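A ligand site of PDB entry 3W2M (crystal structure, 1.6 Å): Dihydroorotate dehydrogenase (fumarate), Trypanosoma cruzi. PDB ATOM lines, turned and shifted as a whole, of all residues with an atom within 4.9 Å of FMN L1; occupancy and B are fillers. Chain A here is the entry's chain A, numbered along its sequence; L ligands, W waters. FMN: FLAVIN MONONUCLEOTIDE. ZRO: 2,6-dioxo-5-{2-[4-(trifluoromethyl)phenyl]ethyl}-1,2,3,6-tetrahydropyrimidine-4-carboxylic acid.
NAO of ZRO L2 sits close to N1 of FMN L1 (3.4 Å).
The side-chain hydroxyl (OG1) of Thr 273 sits at hydrogen-bond distance from the side-chain hydroxyl (OG) of Ser 66 (2.7 Å). The side-chain hydroxyl (OG) of Ser 45 sits at hydrogen-bond distance from the side-chain hydroxyl (OG) of Ser 98 (2.6 Å). The backbone NH (N) of Val 194 is in hydrogen-bond range of the backbone carbonyl oxygen (O) of Cys 249 (2.9 Å). ND2 of Asn 195 sits at hydrogen-bond distance from OD1 of Asn 128, 3.4 Å away. The side-chain amide oxygen of Asn 195 sits at hydrogen-bond distance from the side-chain hydroxyl of Ser 196, at 3.4 Å. N of Ala 19 sits at hydrogen-bond distance from O of Val 271, at 2.9 Å. The side-chain amide oxygen (OD1) of Asn 68 is in hydrogen-bond range of the backbone NH (N) of Met 70 (3.3 Å). The backbone carbonyl oxygen (O) of Gly 222 sits at hydrogen-bond distance from the backbone NH (N) of Ser 66.
Merely in contact with FMN L1: Gly 21, Ala 19, Gly 250, Asn 68, Ile 226, Gly 222, Tyr 59, Met 70 and Ser 196. Of the 30 residues printed, 21 come within 4 Å of FMN L1.
Water W4 lies within hydrogen-bond range of an oxygen (O1P) of FMN L1 (2.7 Å), the backbone NH of Ala 274 (2.9 Å) and the backbone carbonyl oxygen of Val 252 (2.9 Å). Water W3 lies within hydrogen-bond range of OG of Ser 98 (2.6 Å), OE1 of Glu 126 (2.7 Å) and O2 of FMN L1 (2.8 Å). Water W5 lies within hydrogen-bond range of O of Gly 21 (3.0 Å) and NZ of Lys 44 (3.0 Å).
N of Thr 273 lies within hydrogen-bond range of O3P of FMN L1 (2.8 Å). An oxygen (O3P) of FMN L1 lies within hydrogen-bond range of the side-chain hydroxyl (OG1) of Thr 273, 2.7 Å away. N of Gly 223 lies within hydrogen-bond range of O2P of FMN L1, 2.8 Å away. NZ of Lys 44 lies within hydrogen-bond range of O4 of FMN L1. The backbone NH of Ala 20 sits at hydrogen-bond distance from an oxygen (O2') of FMN L1. The backbone carbonyl oxygen (O) of Ala 20 is in hydrogen-bond range of an oxygen (O2') of FMN L1, at 2.8 Å. OG of Ser 45 is in hydrogen-bond range of N3 of FMN L1, at 2.8 Å. The backbone NH of Gly 251 is in hydrogen-bond range of an oxygen (O2P) of FMN L1 (2.8 Å). The side-chain amino group (NZ) of Lys 165 lies within hydrogen-bond range of an oxygen (O2') of FMN L1, at 2.9 Å. N of Gly 272 lies within hydrogen-bond range of O1P of FMN L1, 2.9 Å away. O of Val 194 lies within hydrogen-bond range of O3' of FMN L1, at 3.0 Å. The side-chain amide nitrogen (ND2) of Asn 195 lies within hydrogen-bond range of an oxygen (O2) of FMN L1. The side-chain amide nitrogen of Asn 128 is in hydrogen-bond range of an oxygen (O2) of FMN L1, 3.3 Å away. The side-chain sulfur of Cys 249 lies within hydrogen-bond range of an oxygen (O3') of FMN L1, 3.5 Å away. The side-chain amino group (NZ) of Lys 44 is in salt-bridge range of an oxygen (OAA) of ZRO L2, 3.1 Å away. OD1 of Asn 195 sits at hydrogen-bond distance from NAO of ZRO L2. The side-chain amide nitrogen (ND2) of Asn 128 sits at hydrogen-bond distance from an oxygen (OAC) of ZRO L2 (2.9 Å). An oxygen (OAB) of ZRO L2 sits at hydrogen-bond distance from the side-chain amide nitrogen (ND2) of Asn 68. An oxygen (OAD) of ZRO L2 sits at hydrogen-bond distance from the backbone NH of Met 70 (3.1 Å). An oxygen (OAB) of ZRO L2 lies within hydrogen-bond range of the side-chain hydroxyl of Ser 196 (2.8 Å). The backbone NH (N) of Leu 72 is in hydrogen-bond range of an oxygen (OAA) of ZRO L2 (2.8 Å).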
ATOM      1  N   ALA A  19      25.733   3.552  -0.101  1.00  0.00           N
ATOM      2  CA  ALA A  19      26.403   2.852   0.987  1.00  0.00           C
ATOM      3  C   ALA A  19      27.858   3.234   1.057  1.00  0.00           C
ATOM      4  O   ALA A  19      28.472   3.475   0.035  1.00  0.00           O
ATOM      5  CB  ALA A  19      26.231   1.383   0.762  1.00  0.00           C
ATOM      6  N   ALA A  20      28.385   3.381   2.290  1.00  0.00           N
ATOM      7  CA  ALA A  20      29.743   3.775   2.371  1.00  0.00           C
ATOM      8  C   ALA A  20      30.636   2.837   1.569  1.00  0.00           C
ATOM      9  O   ALA A  20      30.452   1.608   1.559  1.00  0.00           O
ATOM     10  CB  ALA A  20      30.223   3.829   3.822  1.00  0.00           C
ATOM     11  N   GLY A  21      31.601   3.411   0.895  1.00  0.00           N
ATOM     12  CA  GLY A  21      32.481   2.675   0.100  1.00  0.00           C
ATOM     13  C   GLY A  21      32.221   2.730  -1.384  1.00  0.00           C
ATOM     14  O   GLY A  21      33.099   2.419  -2.220  1.00  0.00           O
ATOM     15  N   VAL A  22      30.960   2.925  -1.747  1.00  0.00           N
ATOM     16  CA  VAL A  22      30.548   2.924  -3.152  1.00  0.00           C
ATOM     17  C   VAL A  22      30.333   4.354  -3.619  1.00  0.00           C
ATOM     18  O   VAL A  22      29.627   5.046  -3.023  1.00  0.00           O
ATOM     19  CB  VAL A  22      29.273   2.079  -3.337  1.00  0.00           C
ATOM     20  CG1 VAL A  22      28.798   2.178  -4.768  1.00  0.00           C
ATOM     21  CG2 VAL A  22      29.566   0.668  -2.916  1.00  0.00           C
ATOM     22  N   LYS A  44      33.619   7.613   1.759  1.00  0.00           N
ATOM     23  CA  LYS A  44      34.331   6.388   2.003  1.00  0.00           C
ATOM     24  C   LYS A  44      34.861   6.377   3.442  1.00  0.00           C
ATOM     25  O   LYS A  44      35.491   7.344   3.831  1.00  0.00           O
ATOM     26  CB  LYS A  44      35.485   6.302   0.989  1.00  0.00           C
ATOM     27  CG  LYS A  44      36.436   5.173   1.257  1.00  0.00           C
ATOM     28  CD  LYS A  44      35.939   3.746   1.025  1.00  0.00           C
ATOM     29  CE  LYS A  44      36.827   2.658   1.684  1.00  0.00           C
ATOM     30  NZ  LYS A  44      36.344   1.169   1.468  1.00  0.00           N
ATOM     31  N   SER A  45      34.723   5.238   4.092  1.00  0.00           N
ATOM     32  CA  SER A  45      35.322   5.062   5.445  1.00  0.00           C
ATOM     33  C   SER A  45      36.804   5.414   5.326  1.00  0.00           C
ATOM     34  O   SER A  45      37.499   4.921   4.473  1.00  0.00           O
ATOM     35  CB  SER A  45      35.216   3.694   5.991  1.00  0.00           C
ATOM     36  OG  SER A  45      33.871   3.397   6.289  1.00  0.00           O
ATOM     37  N   TYR A  59      37.275  -6.495  -5.875  1.00  0.00           N
ATOM     38  CA  TYR A  59      35.822  -6.429  -5.976  1.00  0.00           C
ATOM     39  C   TYR A  59      35.428  -7.119  -7.250  1.00  0.00           C
ATOM     40  O   TYR A  59      36.000  -6.890  -8.296  1.00  0.00           O
ATOM     41  CB  TYR A  59      35.344  -4.973  -6.061  1.00  0.00           C
ATOM     42  CG  TYR A  59      33.880  -4.758  -6.399  1.00  0.00           C
ATOM     43  CD1 TYR A  59      33.450  -4.655  -7.696  1.00  0.00           C
ATOM     44  CD2 TYR A  59      32.886  -4.754  -5.413  1.00  0.00           C
ATOM     45  CE1 TYR A  59      32.117  -4.568  -7.994  1.00  0.00           C
ATOM     46  CE2 TYR A  59      31.535  -4.695  -5.725  1.00  0.00           C
ATOM     47  CZ  TYR A  59      31.171  -4.603  -7.052  1.00  0.00           C
ATOM     48  OH  TYR A  59      29.800  -4.398  -7.300  1.00  0.00           O
ATOM     49  N   SER A  66      27.802  -9.255  -4.874  1.00  0.00           N
ATOM     50  CA  SER A  66      29.163  -8.850  -5.014  1.00  0.00           C
ATOM     51  C   SER A  66      29.976  -9.437  -3.804  1.00  0.00           C
ATOM     52  O   SER A  66      29.441  -9.779  -2.774  1.00  0.00           O
ATOM     53  CB  SER A  66      29.354  -7.290  -5.050  1.00  0.00           C
ATOM     54  OG  SER A  66      29.049  -6.756  -3.736  1.00  0.00           O
ATOM     55  N   ASN A  68      33.885  -8.406  -1.865  1.00  0.00           N
ATOM     56  CA  ASN A  68      34.944  -7.403  -1.877  1.00  0.00           C
ATOM     57  C   ASN A  68      35.857  -7.681  -0.688  1.00  0.00           C
ATOM     58  O   ASN A  68      35.442  -7.968   0.430  1.00  0.00           O
ATOM     59  CB  ASN A  68      34.460  -5.987  -1.883  1.00  0.00           C
ATOM     60  CG  ASN A  68      34.188  -5.461  -0.507  1.00  0.00           C
ATOM     61  OD1 ASN A  68      35.109  -4.961   0.198  1.00  0.00           O
ATOM     62  ND2 ASN A  68      32.953  -5.407  -0.137  1.00  0.00           N
ATOM     63  N   MET A  70      38.363  -4.868  -0.182  1.00  0.00           N
ATOM     64  CA  MET A  70      39.023  -3.665  -0.672  1.00  0.00           C
ATOM     65  C   MET A  70      40.247  -3.294   0.160  1.00  0.00           C
ATOM     66  O   MET A  70      41.254  -2.810  -0.358  1.00  0.00           O
ATOM     67  CB  MET A  70      38.080  -2.533  -0.703  1.00  0.00           C
ATOM     68  CG  MET A  70      36.831  -2.562  -1.478  1.00  0.00           C
ATOM     69  SD  MET A  70      37.057  -2.973  -3.205  1.00  0.00           S
ATOM     70  CE  MET A  70      37.567  -1.471  -3.856  1.00  0.00           C
ATOM     71  N   LEU A  72      40.193  -0.983   2.728  1.00  0.00           N
ATOM     72  CA  LEU A  72      40.084   0.389   3.079  1.00  0.00           C
ATOM     73  C   LEU A  72      40.980   1.353   2.285  1.00  0.00           C
ATOM     74  O   LEU A  72      41.581   2.288   2.841  1.00  0.00           O
ATOM     75  CB  LEU A  72      40.365   0.589   4.599  1.00  0.00           C
ATOM     76  CG  LEU A  72      39.544   1.352   5.609  1.00  0.00           C
ATOM     77  CD1 LEU A  72      38.085   1.590   5.335  1.00  0.00           C
ATOM     78  CD2 LEU A  72      39.805   0.727   7.024  1.00  0.00           C
ATOM     79  N   SER A  98      32.071   8.866   6.960  1.00  0.00           N
ATOM     80  CA  SER A  98      32.317   7.616   7.644  1.00  0.00           C
ATOM     81  C   SER A  98      33.740   7.506   8.033  1.00  0.00           C
ATOM     82  O   SER A  98      34.640   7.834   7.234  1.00  0.00           O
ATOM     83  CB  SER A  98      31.969   6.450   6.721  1.00  0.00           C
ATOM     84  OG  SER A  98      32.325   5.183   7.334  1.00  0.00           O
ATOM     85  N   GLU A 126      29.273   8.785  10.678  1.00  0.00           N
ATOM     86  CA  GLU A 126      28.947   7.346  10.709  1.00  0.00           C
ATOM     87  C   GLU A 126      30.247   6.609  11.118  1.00  0.00           C
ATOM     88  O   GLU A 126      31.242   6.617  10.417  1.00  0.00           O
ATOM     89  CB  GLU A 126      28.388   6.854   9.368  1.00  0.00           C
ATOM     90  CG  GLU A 126      27.934   5.384   9.402  1.00  0.00           C
ATOM     91  CD  GLU A 126      27.215   4.874   8.090  1.00  0.00           C
ATOM     92  OE1 GLU A 126      27.936   4.415   7.170  1.00  0.00           O
ATOM     93  OE2 GLU A 126      25.956   4.865   7.878  1.00  0.00           O
ATOM     94  N   ASN A 128      32.275   3.333  11.549  1.00  0.00           N
ATOM     95  CA  ASN A 128      32.241   1.991  11.076  1.00  0.00           C
ATOM     96  C   ASN A 128      32.804   1.020  12.080  1.00  0.00           C
ATOM     97  O   ASN A 128      33.985   1.028  12.304  1.00  0.00           O
ATOM     98  CB  ASN A 128      32.966   1.925   9.773  1.00  0.00           C
ATOM     99  CG  ASN A 128      32.942   0.537   9.163  1.00  0.00           C
ATOM    100  OD1 ASN A 128      32.289  -0.341   9.574  1.00  0.00           O
ATOM    101  ND2 ASN A 128      33.615   0.489   8.004  1.00  0.00           N
ATOM    102  N   LYS A 165      27.783   2.118  11.946  1.00  0.00           N
ATOM    103  CA  LYS A 165      27.558   1.116  10.836  1.00  0.00           C
ATOM    104  C   LYS A 165      27.906  -0.268  11.463  1.00  0.00           C
ATOM    105  O   LYS A 165      28.999  -0.496  11.979  1.00  0.00           O
ATOM    106  CB  LYS A 165      28.470   1.373   9.691  1.00  0.00           C
ATOM    107  CG  LYS A 165      28.381   0.401   8.487  1.00  0.00           C
ATOM    108  CD  LYS A 165      27.154   0.531   7.670  1.00  0.00           C
ATOM    109  CE  LYS A 165      27.242  -0.259   6.420  1.00  0.00           C
ATOM    110  NZ  LYS A 165      28.138   0.367   5.438  1.00  0.00           N
ATOM    111  N   VAL A 194      22.944  -3.154   7.226  1.00  0.00           N
ATOM    112  CA  VAL A 194      24.148  -3.843   7.690  1.00  0.00           C
ATOM    113  C   VAL A 194      25.321  -3.624   6.734  1.00  0.00           C
ATOM    114  O   VAL A 194      25.141  -3.267   5.632  1.00  0.00           O
ATOM    115  CB  VAL A 194      23.966  -5.388   7.787  1.00  0.00           C
ATOM    116  CG1 VAL A 194      22.940  -5.723   8.807  1.00  0.00           C
ATOM    117  CG2 VAL A 194      23.602  -6.004   6.424  1.00  0.00           C
ATOM    118  N   ASN A 195      26.516  -3.842   7.248  1.00  0.00           N
ATOM    119  CA  ASN A 195      27.687  -3.921   6.412  1.00  0.00           C
ATOM    120  C   ASN A 195      27.639  -5.305   5.726  1.00  0.00           C
ATOM    121  O   ASN A 195      26.750  -5.994   5.904  1.00  0.00           O
ATOM    122  CB  ASN A 195      28.919  -3.801   7.305  1.00  0.00           C
ATOM    123  CG  ASN A 195      30.097  -3.199   6.601  1.00  0.00           C
ATOM    124  OD1 ASN A 195      30.453  -3.602   5.572  1.00  0.00           O
ATOM    125  ND2 ASN A 195      30.679  -2.218   7.220  1.00  0.00           N
ATOM    126  N   SER A 196      28.672  -5.612   4.973  1.00  0.00           N
ATOM    127  CA  SER A 196      28.653  -6.837   4.209  1.00  0.00           C
ATOM    128  C   SER A 196      28.597  -8.101   5.062  1.00  0.00           C
ATOM    129  O   SER A 196      28.968  -8.093   6.167  1.00  0.00           O
ATOM    130  CB  SER A 196      29.838  -6.856   3.203  1.00  0.00           C
ATOM    131  OG  SER A 196      31.014  -6.451   3.749  1.00  0.00           O
ATOM    132  N   GLY A 222      27.738  -8.625  -0.608  1.00  0.00           N
ATOM    133  CA  GLY A 222      26.625  -7.699  -0.738  1.00  0.00           C
ATOM    134  C   GLY A 222      25.679  -8.153  -1.850  1.00  0.00           C
ATOM    135  O   GLY A 222      25.956  -9.083  -2.593  1.00  0.00           O
ATOM    136  N   GLY A 223      24.596  -7.433  -1.929  1.00  0.00           N
ATOM    137  CA  GLY A 223      23.652  -7.592  -2.974  1.00  0.00           C
ATOM    138  C   GLY A 223      22.474  -8.529  -2.644  1.00  0.00           C
ATOM    139  O   GLY A 223      22.047  -8.677  -1.476  1.00  0.00           O
ATOM    140  N   ILE A 226      22.071 -10.939   0.401  1.00  0.00           N
ATOM    141  CA  ILE A 226      22.031 -10.548   1.770  1.00  0.00           C
ATOM    142  C   ILE A 226      20.757  -9.825   2.183  1.00  0.00           C
ATOM    143  O   ILE A 226      20.631  -9.428   3.338  1.00  0.00           O
ATOM    144  CB  ILE A 226      23.266  -9.690   2.149  1.00  0.00           C
ATOM    145  CG1 ILE A 226      23.203  -8.230   1.680  1.00  0.00           C
ATOM    146  CG2 ILE A 226      24.548 -10.395   1.722  1.00  0.00           C
ATOM    147  CD1 ILE A 226      24.173  -7.278   2.431  1.00  0.00           C
ATOM    148  N   CYS A 249      20.629  -0.984   5.000  1.00  0.00           N
ATOM    149  CA  CYS A 249      21.631  -1.221   3.933  1.00  0.00           C
ATOM    150  C   CYS A 249      21.687  -2.698   3.671  1.00  0.00           C
ATOM    151  O   CYS A 249      21.782  -3.479   4.623  1.00  0.00           O
ATOM    152  CB  CYS A 249      22.962  -0.671   4.344  1.00  0.00           C
ATOM    153  SG  CYS A 249      24.179  -0.672   3.028  1.00  0.00           S
ATOM    154  N   GLY A 250      21.558  -3.137   2.411  1.00  0.00           N
ATOM    155  CA  GLY A 250      21.797  -4.496   1.990  1.00  0.00           C
ATOM    156  C   GLY A 250      20.737  -4.977   1.051  1.00  0.00           C
ATOM    157  O   GLY A 250      19.569  -5.001   1.402  1.00  0.00           O
ATOM    158  N   GLY A 251      21.203  -5.349  -0.127  1.00  0.00           N
ATOM    159  CA  GLY A 251      20.300  -6.014  -1.082  1.00  0.00           C
ATOM    160  C   GLY A 251      19.330  -5.143  -1.760  1.00  0.00           C
ATOM    161  O   GLY A 251      18.358  -5.689  -2.334  1.00  0.00           O
ATOM    162  N   VAL A 252      19.473  -3.805  -1.720  1.00  0.00           N
ATOM    163  CA  VAL A 252      18.488  -2.925  -2.424  1.00  0.00           C
ATOM    164  C   VAL A 252      18.839  -2.805  -3.898  1.00  0.00           C
ATOM    165  O   VAL A 252      19.855  -2.198  -4.233  1.00  0.00           O
ATOM    166  CB  VAL A 252      18.397  -1.541  -1.752  1.00  0.00           C
ATOM    167  CG1 VAL A 252      17.461  -0.640  -2.510  1.00  0.00           C
ATOM    168  CG2 VAL A 252      17.911  -1.657  -0.305  1.00  0.00           C
ATOM    169  N   GLN A 270      20.234   2.731   2.144  1.00  0.00           N
ATOM    170  CA  GLN A 270      21.541   2.886   1.468  1.00  0.00           C
ATOM    171  C   GLN A 270      21.619   1.775   0.375  1.00  0.00           C
ATOM    172  O   GLN A 270      21.048   0.695   0.529  1.00  0.00           O
ATOM    173  CB  GLN A 270      22.695   2.733   2.472  1.00  0.00           C
ATOM    174  CG  GLN A 270      22.556   3.614   3.658  1.00  0.00           C
ATOM    175  CD  GLN A 270      23.827   3.562   4.499  1.00  0.00           C
ATOM    176  OE1 GLN A 270      24.579   2.588   4.496  1.00  0.00           O
ATOM    177  NE2 GLN A 270      24.014   4.572   5.319  1.00  0.00           N
ATOM    178  N   VAL A 271      22.381   2.074  -0.680  1.00  0.00           N
ATOM    179  CA  VAL A 271      22.503   1.305  -1.912  1.00  0.00           C
ATOM    180  C   VAL A 271      24.005   1.167  -2.184  1.00  0.00           C
ATOM    181  O   VAL A 271      24.675   2.157  -2.460  1.00  0.00           O
ATOM    182  CB  VAL A 271      21.737   1.940  -3.045  1.00  0.00           C
ATOM    183  CG1 VAL A 271      21.727   1.002  -4.196  1.00  0.00           C
ATOM    184  CG2 VAL A 271      20.336   2.394  -2.652  1.00  0.00           C
ATOM    185  N   GLY A 272      24.475  -0.061  -2.105  1.00  0.00           N
ATOM    186  CA  GLY A 272      25.890  -0.473  -2.339  1.00  0.00           C
ATOM    187  C   GLY A 272      26.024  -1.105  -3.686  1.00  0.00           C
ATOM    188  O   GLY A 272      26.182  -0.450  -4.697  1.00  0.00           O
ATOM    189  N   THR A 273      26.057  -2.444  -3.684  1.00  0.00           N
ATOM    190  CA  THR A 273      26.285  -3.208  -4.888  1.00  0.00           C
ATOM    191  C   THR A 273      25.468  -2.746  -6.086  1.00  0.00           C
ATOM    192  O   THR A 273      25.998  -2.564  -7.146  1.00  0.00           O
ATOM    193  CB  THR A 273      25.926  -4.687  -4.600  1.00  0.00           C
ATOM    194  OG1 THR A 273      26.856  -5.186  -3.596  1.00  0.00           O
ATOM    195  CG2 THR A 273      26.144  -5.513  -5.788  1.00  0.00           C
ATOM    196  N   ALA A 274      24.185  -2.531  -5.912  1.00  0.00           N
ATOM    197  CA  ALA A 274      23.369  -2.153  -7.067  1.00  0.00           C
ATOM    198  C   ALA A 274      23.804  -0.814  -7.664  1.00  0.00           C
ATOM    199  O   ALA A 274      23.653  -0.603  -8.867  1.00  0.00           O
ATOM    200  CB  ALA A 274      21.870  -2.050  -6.666  1.00  0.00           C
HETATM  201  N1  FMN L   1      31.003  -0.224   4.286  1.00  0.00           N
HETATM  202  C2  FMN L   1      31.547   0.697   5.131  1.00  0.00           C
HETATM  203  O2  FMN L   1      30.899   1.012   6.159  1.00  0.00           O
HETATM  204  N3  FMN L   1      32.660   1.377   4.797  1.00  0.00           N
HETATM  205  C4  FMN L   1      33.359   1.149   3.658  1.00  0.00           C
HETATM  206  O4  FMN L   1      34.390   1.827   3.327  1.00  0.00           O
HETATM  207  C4A FMN L   1      32.862   0.171   2.747  1.00  0.00           C
HETATM  208  N5  FMN L   1      33.483  -0.086   1.589  1.00  0.00           N
HETATM  209  C5A FMN L   1      32.872  -0.934   0.676  1.00  0.00           C
HETATM  210  C6  FMN L   1      33.380  -1.037  -0.617  1.00  0.00           C
HETATM  211  C7  FMN L   1      32.767  -1.819  -1.595  1.00  0.00           C
HETATM  212  C7M FMN L   1      33.399  -1.966  -2.956  1.00  0.00           C
HETATM  213  C8  FMN L   1      31.539  -2.508  -1.286  1.00  0.00           C
HETATM  214  C8M FMN L   1      30.834  -3.350  -2.266  1.00  0.00           C
HETATM  215  C9  FMN L   1      30.990  -2.320  -0.017  1.00  0.00           C
HETATM  216  C9A FMN L   1      31.610  -1.582   0.979  1.00  0.00           C
HETATM  217  N10 FMN L   1      31.097  -1.408   2.286  1.00  0.00           N
HETATM  218  C10 FMN L   1      31.616  -0.477   3.142  1.00  0.00           C
HETATM  219  C1' FMN L   1      29.851  -2.047   2.637  1.00  0.00           C
HETATM  220  C2' FMN L   1      28.605  -1.376   2.060  1.00  0.00           C
HETATM  221  O2' FMN L   1      28.532  -0.079   2.647  1.00  0.00           O
HETATM  222  C3' FMN L   1      27.339  -2.141   2.332  1.00  0.00           C
HETATM  223  O3' FMN L   1      27.186  -2.187   3.793  1.00  0.00           O
HETATM  224  C4' FMN L   1      27.330  -3.560   1.803  1.00  0.00           C
HETATM  225  O4' FMN L   1      27.875  -3.530   0.471  1.00  0.00           O
HETATM  226  C5' FMN L   1      25.911  -4.082   1.683  1.00  0.00           C
HETATM  227  O5' FMN L   1      25.011  -3.344   0.930  1.00  0.00           O
HETATM  228  P   FMN L   1      24.623  -3.818  -0.598  1.00  0.00           P
HETATM  229  O1P FMN L   1      23.763  -2.725  -1.160  1.00  0.00           O
HETATM  230  O2P FMN L   1      23.974  -5.155  -0.475  1.00  0.00           O
HETATM  231  O3P FMN L   1      25.979  -3.992  -1.342  1.00  0.00           O
HETATM  232  OAA ZRO L   2      37.415  -1.468   2.629  1.00  0.00           O
HETATM  233  CAP ZRO L   2      36.872  -2.563   2.749  1.00  0.00           C
HETATM  234  OAD ZRO L   2      37.341  -3.651   2.499  1.00  0.00           O
HETATM  235  CAS ZRO L   2      35.486  -2.648   3.406  1.00  0.00           C
HETATM  236  NAN ZRO L   2      34.564  -3.404   2.710  1.00  0.00           N
HETATM  237  CAU ZRO L   2      33.292  -3.624   3.173  1.00  0.00           C
HETATM  238  OAB ZRO L   2      32.487  -4.418   2.589  1.00  0.00           O
HETATM  239  NAO ZRO L   2      32.918  -3.071   4.354  1.00  0.00           N
HETATM  240  CAV ZRO L   2      33.828  -2.301   5.120  1.00  0.00           C
HETATM  241  OAC ZRO L   2      33.420  -1.758   6.162  1.00  0.00           O
HETATM  242  CAT ZRO L   2      35.147  -2.141   4.614  1.00  0.00           C
HETATM  243  CAM ZRO L   2      36.022  -1.339   5.364  1.00  0.00           C
HETATM  244  CAL ZRO L   2      36.487  -2.083   6.698  1.00  0.00           C
HETATM  245  CAQ ZRO L   2      37.333  -3.144   6.378  1.00  0.00           C
HETATM  246  CAH ZRO L   2      38.693  -3.008   6.204  1.00  0.00           C
HETATM  247  CAJ ZRO L   2      39.542  -4.078   5.827  1.00  0.00           C
HETATM  248  CAR ZRO L   2      39.001  -5.326   5.430  1.00  0.00           C
HETATM  249  CAW ZRO L   2      39.824  -6.443   4.889  1.00  0.00           C
HETATM  250  FAF ZRO L   2      41.138  -6.257   4.989  1.00  0.00           F
HETATM  251  FAG ZRO L   2      39.438  -7.650   5.420  1.00  0.00           F
HETATM  252  FAE ZRO L   2      39.703  -6.388   3.364  1.00  0.00           F
HETATM  253  CAK ZRO L   2      37.600  -5.470   5.556  1.00  0.00           C
HETATM  254  CAI ZRO L   2      36.795  -4.418   6.066  1.00  0.00           C
HETATM  255  O   HOH W   1      29.356  -5.660   0.562  1.00  0.00           O
HETATM  256  O   HOH W   2      21.397  -1.974  -0.221  1.00  0.00           O
HETATM  257  O   HOH W   3      30.404   3.429   7.567  1.00  0.00           O
HETATM  258  O   HOH W   4      22.582  -3.038  -3.579  1.00  0.00           O
HETATM  259  O   HOH W   5      35.770   1.259  -1.510  1.00  0.00           O
